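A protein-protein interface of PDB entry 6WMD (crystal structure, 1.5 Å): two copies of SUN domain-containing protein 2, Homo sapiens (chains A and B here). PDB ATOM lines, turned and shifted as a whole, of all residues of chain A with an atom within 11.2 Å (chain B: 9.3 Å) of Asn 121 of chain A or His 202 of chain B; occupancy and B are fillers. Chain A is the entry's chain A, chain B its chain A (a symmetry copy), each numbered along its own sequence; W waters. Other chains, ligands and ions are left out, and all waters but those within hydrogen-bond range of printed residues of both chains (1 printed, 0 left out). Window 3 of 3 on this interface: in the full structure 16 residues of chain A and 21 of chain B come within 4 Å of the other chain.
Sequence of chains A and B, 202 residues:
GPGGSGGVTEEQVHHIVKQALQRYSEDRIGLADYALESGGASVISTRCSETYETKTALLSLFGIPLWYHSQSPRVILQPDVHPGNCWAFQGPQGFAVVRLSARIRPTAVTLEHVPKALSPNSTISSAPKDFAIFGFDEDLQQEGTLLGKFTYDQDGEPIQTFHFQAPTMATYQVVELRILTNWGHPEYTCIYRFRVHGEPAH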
ATOM      1  N   VAL A 114     -10.423  22.297  40.211  1.00  0.00           N
ATOM      2  CA  VAL A 114     -10.561  20.955  39.637  1.00  0.00           C
ATOM      3  C   VAL A 114      -9.200  20.406  39.220  1.00  0.00           C
ATOM      4  O   VAL A 114      -8.297  21.180  38.876  1.00  0.00           O
ATOM      5  CB  VAL A 114     -11.557  20.934  38.468  1.00  0.00           C
ATOM      6  CG1 VAL A 114     -12.969  21.110  39.000  1.00  0.00           C
ATOM      7  CG2 VAL A 114     -11.198  21.991  37.423  1.00  0.00           C
ATOM      8  N   PRO A 115      -9.013  19.089  39.229  1.00  0.00           N
ATOM      9  CA  PRO A 115      -7.717  18.517  38.845  1.00  0.00           C
ATOM     10  C   PRO A 115      -7.466  18.592  37.346  1.00  0.00           C
ATOM     11  O   PRO A 115      -8.387  18.521  36.527  1.00  0.00           O
ATOM     12  CB  PRO A 115      -7.826  17.048  39.269  1.00  0.00           C
ATOM     13  CG  PRO A 115      -9.127  16.891  39.972  1.00  0.00           C
ATOM     14  CD  PRO A 115      -9.972  18.093  39.735  1.00  0.00           C
ATOM     15  N   LYS A 116      -6.176  18.644  36.990  1.00  0.00           N
ATOM     16  CA  LYS A 116      -5.789  18.557  35.583  1.00  0.00           C
ATOM     17  C   LYS A 116      -6.330  17.293  34.924  1.00  0.00           C
ATOM     18  O   LYS A 116      -6.690  17.311  33.743  1.00  0.00           O
ATOM     19  CB  LYS A 116      -4.263  18.564  35.442  1.00  0.00           C
ATOM     20  CG  LYS A 116      -3.576  19.877  35.721  1.00  0.00           C
ATOM     21  CD  LYS A 116      -2.082  19.668  35.499  1.00  0.00           C
ATOM     22  CE  LYS A 116      -1.272  20.935  35.712  1.00  0.00           C
ATOM     23  NZ  LYS A 116       0.195  20.583  35.843  1.00  0.00           N
ATOM     24  N   ALA A 117      -6.366  16.172  35.657  1.00  0.00           N
ATOM     25  CA  ALA A 117      -6.797  14.914  35.058  1.00  0.00           C
ATOM     26  C   ALA A 117      -8.252  14.945  34.610  1.00  0.00           C
ATOM     27  O   ALA A 117      -8.632  14.126  33.762  1.00  0.00           O
ATOM     28  CB  ALA A 117      -6.596  13.757  36.042  1.00  0.00           C
ATOM     29  N   LEU A 118      -9.060  15.867  35.152  1.00  0.00           N
ATOM     30  CA  LEU A 118     -10.461  16.010  34.769  1.00  0.00           C
ATOM     31  C   LEU A 118     -10.677  17.182  33.821  1.00  0.00           C
ATOM     32  O   LEU A 118     -11.826  17.552  33.546  1.00  0.00           O
ATOM     33  CB  LEU A 118     -11.342  16.151  36.013  1.00  0.00           C
ATOM     34  CG  LEU A 118     -11.240  14.948  36.959  1.00  0.00           C
ATOM     35  CD1 LEU A 118     -12.221  15.159  38.113  1.00  0.00           C
ATOM     36  CD2 LEU A 118     -11.541  13.659  36.224  1.00  0.00           C
ATOM     37  N   SER A 119      -9.600  17.736  33.273  1.00  0.00           N
ATOM     38  CA  SER A 119      -9.657  18.931  32.446  1.00  0.00           C
ATOM     39  C   SER A 119      -9.225  18.631  31.017  1.00  0.00           C
ATOM     40  O   SER A 119      -8.246  17.910  30.809  1.00  0.00           O
ATOM     41  CB  SER A 119      -8.697  19.969  33.035  1.00  0.00           C
ATOM     42  OG  SER A 119      -9.096  20.313  34.347  1.00  0.00           O
ATOM     43  N   PRO A 120      -9.919  19.171  30.017  1.00  0.00           N
ATOM     44  CA  PRO A 120      -9.461  19.034  28.629  1.00  0.00           C
ATOM     45  C   PRO A 120      -8.026  19.525  28.489  1.00  0.00           C
ATOM     46  O   PRO A 120      -7.658  20.586  29.000  1.00  0.00           O
ATOM     47  CB  PRO A 120     -10.434  19.930  27.850  1.00  0.00           C
ATOM     48  CG  PRO A 120     -11.688  19.931  28.701  1.00  0.00           C
ATOM     49  CD  PRO A 120     -11.227  19.847  30.131  1.00  0.00           C
ATOM     50  N   ASN A 121      -7.201  18.732  27.814  1.00  0.00           N
ATOM     51  CA  ASN A 121      -5.792  19.042  27.579  1.00  0.00           C
ATOM     52  C   ASN A 121      -4.967  19.161  28.853  1.00  0.00           C
ATOM     53  O   ASN A 121      -3.832  19.656  28.805  1.00  0.00           O
ATOM     54  CB  ASN A 121      -5.603  20.268  26.683  1.00  0.00           C
ATOM     55  CG  ASN A 121      -6.060  20.004  25.275  1.00  0.00           C
ATOM     56  OD1 ASN A 121      -5.654  19.016  24.653  1.00  0.00           O
ATOM     57  ND2 ASN A 121      -6.919  20.868  24.763  1.00  0.00           N
ATOM     58  N   SER A 122      -5.505  18.716  29.995  1.00  0.00           N
ATOM     59  CA  SER A 122      -4.766  18.696  31.251  1.00  0.00           C
ATOM     60  C   SER A 122      -4.334  20.090  31.685  1.00  0.00           C
ATOM     61  O   SER A 122      -3.309  20.242  32.357  1.00  0.00           O
ATOM     62  CB  SER A 122      -3.570  17.735  31.211  1.00  0.00           C
ATOM     63  OG  SER A 122      -4.013  16.400  31.015  1.00  0.00           O
ATOM     64  N   THR A 123      -5.106  21.122  31.320  1.00  0.00           N
ATOM     65  CA  THR A 123      -4.770  22.491  31.712  1.00  0.00           C
ATOM     66  C   THR A 123      -5.874  23.114  32.557  1.00  0.00           C
ATOM     67  O   THR A 123      -7.065  22.854  32.351  1.00  0.00           O
ATOM     68  CB  THR A 123      -4.490  23.387  30.497  1.00  0.00           C
ATOM     69  OG1 THR A 123      -5.622  23.387  29.620  1.00  0.00           O
ATOM     70  CG2 THR A 123      -3.251  22.892  29.733  1.00  0.00           C
ATOM     71  N   ILE A 124      -5.456  23.968  33.503  1.00  0.00           N
ATOM     72  CA  ILE A 124      -6.374  24.672  34.403  1.00  0.00           C
ATOM     73  C   ILE A 124      -6.032  26.159  34.420  1.00  0.00           C
ATOM     74  O   ILE A 124      -5.852  26.758  35.491  1.00  0.00           O
ATOM     75  CB  ILE A 124      -6.389  24.065  35.820  1.00  0.00           C
ATOM     76  CG1 ILE A 124      -4.972  23.892  36.379  1.00  0.00           C
ATOM     77  CG2 ILE A 124      -7.121  22.727  35.802  1.00  0.00           C
ATOM     78  CD1 ILE A 124      -4.959  23.562  37.863  1.00  0.00           C
ATOM     79  N   SER A 125      -5.972  26.771  33.237  1.00  0.00           N
ATOM     80  CA  SER A 125      -5.517  28.155  33.126  1.00  0.00           C
ATOM     81  C   SER A 125      -6.456  29.159  33.792  1.00  0.00           C
ATOM     82  O   SER A 125      -6.019  30.276  34.095  1.00  0.00           O
ATOM     83  CB  SER A 125      -5.295  28.518  31.663  1.00  0.00           C
ATOM     84  OG  SER A 125      -6.527  28.624  30.968  1.00  0.00           O
ATOM     85  N   GLN A 154      -0.669  25.749  40.151  1.00  0.00           N
ATOM     86  CA  GLN A 154      -1.374  24.908  39.191  1.00  0.00           C
ATOM     87  C   GLN A 154      -0.750  23.526  39.066  1.00  0.00           C
ATOM     88  O   GLN A 154      -1.425  22.610  38.579  1.00  0.00           O
ATOM     89  CB  GLN A 154      -1.444  25.575  37.809  1.00  0.00           C
ATOM     90  CG  GLN A 154      -0.082  25.747  37.135  1.00  0.00           C
ATOM     91  CD  GLN A 154      -0.178  26.000  35.638  1.00  0.00           C
ATOM     92  OE1 GLN A 154      -1.271  26.127  35.076  1.00  0.00           O
ATOM     93  NE2 GLN A 154       0.977  26.109  34.990  1.00  0.00           N
ATOM     94  N   ASP A 155       0.514  23.356  39.477  1.00  0.00           N
ATOM     95  CA  ASP A 155       1.185  22.061  39.396  1.00  0.00           C
ATOM     96  C   ASP A 155       1.095  21.280  40.692  1.00  0.00           C
ATOM     97  O   ASP A 155       1.673  20.188  40.787  1.00  0.00           O
ATOM     98  CB  ASP A 155       2.661  22.221  38.998  1.00  0.00           C
ATOM     99  CG  ASP A 155       2.848  22.736  37.568  1.00  0.00           C
ATOM    100  OD1 ASP A 155       1.908  22.650  36.743  1.00  0.00           O
ATOM    101  OD2 ASP A 155       3.962  23.247  37.270  1.00  0.00           O
ATOM    102  N   HIS A 185      -5.776  32.243  31.801  1.00  0.00           N
ATOM    103  CA  HIS A 185      -6.989  32.244  31.000  1.00  0.00           C
ATOM    104  C   HIS A 185      -7.295  33.667  30.549  1.00  0.00           C
ATOM    105  O   HIS A 185      -7.323  34.584  31.380  1.00  0.00           O
ATOM    106  CB  HIS A 185      -8.183  31.683  31.764  1.00  0.00           C
ATOM    107  CG  HIS A 185      -9.306  31.274  30.868  1.00  0.00           C
ATOM    108  ND1 HIS A 185     -10.147  32.185  30.263  1.00  0.00           N
ATOM    109  CD2 HIS A 185      -9.709  30.050  30.450  1.00  0.00           C
ATOM    110  CE1 HIS A 185     -11.021  31.537  29.512  1.00  0.00           C
ATOM    111  NE2 HIS A 185     -10.780  30.241  29.612  1.00  0.00           N
ATOM    112  N   ALA B  32     -11.217  12.993  31.947  1.00  0.00           N
ATOM    113  CA  ALA B  32     -12.179  14.067  31.737  1.00  0.00           C
ATOM    114  C   ALA B  32     -13.444  13.522  31.091  1.00  0.00           C
ATOM    115  O   ALA B  32     -13.396  12.614  30.253  1.00  0.00           O
ATOM    116  CB  ALA B  32     -11.582  15.165  30.856  1.00  0.00           C
ATOM    117  N   TYR B  34     -16.603  14.448  28.889  1.00  0.00           N
ATOM    118  CA  TYR B  34     -17.203  15.400  27.961  1.00  0.00           C
ATOM    119  C   TYR B  34     -18.723  15.315  27.946  1.00  0.00           C
ATOM    120  O   TYR B  34     -19.373  16.125  27.273  1.00  0.00           O
ATOM    121  CB  TYR B  34     -16.599  15.226  26.551  1.00  0.00           C
ATOM    122  CG  TYR B  34     -15.140  15.600  26.571  1.00  0.00           C
ATOM    123  CD1 TYR B  34     -14.745  16.926  26.419  1.00  0.00           C
ATOM    124  CD2 TYR B  34     -14.163  14.648  26.855  1.00  0.00           C
ATOM    125  CE1 TYR B  34     -13.407  17.282  26.505  1.00  0.00           C
ATOM    126  CE2 TYR B  34     -12.819  15.000  26.944  1.00  0.00           C
ATOM    127  CZ  TYR B  34     -12.455  16.315  26.770  1.00  0.00           C
ATOM    128  OH  TYR B  34     -11.121  16.669  26.868  1.00  0.00           O
ATOM    129  N   ALA B 102     -17.666  19.436  24.153  1.00  0.00           N
ATOM    130  CA  ALA B 102     -16.732  19.815  23.105  1.00  0.00           C
ATOM    131  C   ALA B 102     -16.714  18.714  22.061  1.00  0.00           C
ATOM    132  O   ALA B 102     -17.073  17.566  22.333  1.00  0.00           O
ATOM    133  CB  ALA B 102     -15.318  20.035  23.667  1.00  0.00           C
ATOM    134  N   ARG B 103     -16.297  19.090  20.853  1.00  0.00           N
ATOM    135  CA  ARG B 103     -16.063  18.119  19.794  1.00  0.00           C
ATOM    136  C   ARG B 103     -14.781  17.346  20.091  1.00  0.00           C
ATOM    137  O   ARG B 103     -13.722  17.946  20.318  1.00  0.00           O
ATOM    138  CB  ARG B 103     -15.927  18.876  18.474  1.00  0.00           C
ATOM    139  CG  ARG B 103     -15.517  18.020  17.294  1.00  0.00           C
ATOM    140  CD  ARG B 103     -15.657  18.799  15.989  1.00  0.00           C
ATOM    141  NE  ARG B 103     -17.064  18.964  15.659  1.00  0.00           N
ATOM    142  CZ  ARG B 103     -17.779  18.066  14.988  1.00  0.00           C
ATOM    143  NH1 ARG B 103     -17.208  16.947  14.565  1.00  0.00           N
ATOM    144  NH2 ARG B 103     -19.063  18.289  14.742  1.00  0.00           N
ATOM    145  N   ILE B 104     -14.870  16.011  20.105  1.00  0.00           N
ATOM    146  CA  ILE B 104     -13.738  15.168  20.478  1.00  0.00           C
ATOM    147  C   ILE B 104     -13.634  13.973  19.542  1.00  0.00           C
ATOM    148  O   ILE B 104     -14.583  13.609  18.846  1.00  0.00           O
ATOM    149  CB  ILE B 104     -13.823  14.627  21.927  1.00  0.00           C
ATOM    150  CG1 ILE B 104     -15.023  13.682  22.061  1.00  0.00           C
ATOM    151  CG2 ILE B 104     -13.905  15.759  22.944  1.00  0.00           C
ATOM    152  CD1 ILE B 104     -15.157  13.067  23.461  1.00  0.00           C
ATOM    153  N   MET B 169     -10.026   8.757  13.267  1.00  0.00           N
ATOM    154  CA  MET B 169      -9.721  10.164  13.470  1.00  0.00           C
ATOM    155  C   MET B 169     -10.963  11.045  13.443  1.00  0.00           C
ATOM    156  O   MET B 169     -10.842  12.260  13.635  1.00  0.00           O
ATOM    157  CB  MET B 169      -8.714  10.644  12.419  1.00  0.00           C
ATOM    158  CG  MET B 169      -7.336  10.014  12.559  1.00  0.00           C
ATOM    159  SD  MET B 169      -6.596  10.301  14.181  1.00  0.00           S
ATOM    160  CE  MET B 169      -6.134  12.028  14.047  1.00  0.00           C
ATOM    161  N   GLY B 198     -12.341  11.275  25.638  1.00  0.00           N
ATOM    162  CA  GLY B 198     -11.659  11.330  24.358  1.00  0.00           C
ATOM    163  C   GLY B 198     -10.706  12.503  24.256  1.00  0.00           C
ATOM    164  O   GLY B 198     -10.331  13.116  25.256  1.00  0.00           O
ATOM    165  N   GLU B 199     -10.325  12.794  23.017  1.00  0.00           N
ATOM    166  CA  GLU B 199      -9.269  13.751  22.715  1.00  0.00           C
ATOM    167  C   GLU B 199      -9.884  15.016  22.130  1.00  0.00           C
ATOM    168  O   GLU B 199     -10.442  14.974  21.018  1.00  0.00           O
ATOM    169  CB  GLU B 199      -8.303  13.120  21.712  1.00  0.00           C
ATOM    170  CG  GLU B 199      -7.484  11.986  22.313  1.00  0.00           C
ATOM    171  CD  GLU B 199      -6.624  11.256  21.296  1.00  0.00           C
ATOM    172  OE1 GLU B 199      -6.473  11.757  20.159  1.00  0.00           O
ATOM    173  OE2 GLU B 199      -6.100  10.174  21.640  1.00  0.00           O
ATOM    174  N   PRO B 200      -9.803  16.149  22.813  1.00  0.00           N
ATOM    175  CA  PRO B 200     -10.344  17.401  22.278  1.00  0.00           C
ATOM    176  C   PRO B 200      -9.344  18.049  21.328  1.00  0.00           C
ATOM    177  O   PRO B 200      -8.226  17.573  21.122  1.00  0.00           O
ATOM    178  CB  PRO B 200     -10.509  18.251  23.543  1.00  0.00           C
ATOM    179  CG  PRO B 200      -9.320  17.837  24.386  1.00  0.00           C
ATOM    180  CD  PRO B 200      -9.190  16.332  24.145  1.00  0.00           C
ATOM    181  N   ALA B 201      -9.767  19.164  20.742  1.00  0.00           N
ATOM    182  CA  ALA B 201      -8.857  19.982  19.964  1.00  0.00           C
ATOM    183  C   ALA B 201      -7.786  20.574  20.874  1.00  0.00           C
ATOM    184  O   ALA B 201      -7.986  20.739  22.079  1.00  0.00           O
ATOM    185  CB  ALA B 201      -9.632  21.111  19.291  1.00  0.00           C
ATOM    186  N   HIS B 202      -6.630  20.869  20.299  1.00  0.00           N
ATOM    187  CA  HIS B 202      -5.598  21.563  21.064  1.00  0.00           C
ATOM    188  C   HIS B 202      -4.857  22.576  20.212  1.00  0.00           C
ATOM    189  O   HIS B 202      -5.138  22.727  19.018  1.00  0.00           O
ATOM    190  CB  HIS B 202      -4.620  20.577  21.716  1.00  0.00           C
ATOM    191  CG  HIS B 202      -3.805  19.791  20.739  1.00  0.00           C
ATOM    192  ND1 HIS B 202      -4.277  18.654  20.119  1.00  0.00           N
ATOM    193  CD2 HIS B 202      -2.542  19.970  20.284  1.00  0.00           C
ATOM    194  CE1 HIS B 202      -3.343  18.172  19.317  1.00  0.00           C
ATOM    195  NE2 HIS B 202      -2.280  18.952  19.399  1.00  0.00           N
ATOM    196  OXT HIS B 202      -3.968  23.273  20.708  1.00  0.00           O
HETATM  197  O   HOH W   1      -6.021  17.131  22.755  1.00  0.00           O
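Asn 121 of chain A touches three residues of chain B. His 202 of chain B touches just one residue of chain A: Asn 121 (3.5 Å). No residue of chain B comes within 4 Å of Ser 122 of chain A. Of the printed residues of chain A, Ala 201 of chain B touches Asn 121 (2.9 Å). Of the printed residues of chain A, Tyr 34 of chain B touches Pro 120. Printed residues of chain B within 4 Å of Ala 117 of chain A: Ala 32. Thr 123 of chain A touches none of the printed residues of chain B. The nearest residue of chain A that does not touch His 202 of chain B is Pro 120 of chain A (7.7 Å). The nearest printed residue of chain A that does not touch Tyr 34 of chain B is Asn 121 of chain A (4.5 Å).
Ala 32 of chain B touches Leu 118 of chain A (CB to O, 3.6 Å). Pro 120 of chain A touches Tyr 34 of chain B (CA to OH, 3.4 Å). Asn 121 of chain A touches Pro 200 of chain B. Asn 121 of chain A touches His 202 of chain B.
No position is printed for both chains. Of the 6 pairs that touch across the chains among the printed residues, none has its exchanged pair printed and touching as well.
Water W1 bridges the side-chain amide oxygen of Asn 121 of chain A (2.7 Å) and the backbone carbonyl oxygen of Pro 200 of chain B (2.8 Å).
Of the 11 printed residues of chain B, 5 touch a printed residue of chain A. Printed residues of chain B that touch a printed residue of chain A: Ala 32, Tyr 34, Pro 200, Ala 201 and His 202. Hydrophobic or aromatic side chains of chain B that line the printed part of chain A: Ala 32, Tyr 34, Pro 200 and His 202. Of the 15 printed residues of chain A, 4 touch a printed residue of chain B.
O of Ala 117 of chain A is in hydrogen-bond range of N of Ala 32 of chain B (3.4 Å). The side-chain amide nitrogen (ND2) of Asn 121 of chain A lies within hydrogen-bond range of the backbone carbonyl oxygen (O) of Ala 201 of chain B, at 2.9 Å.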
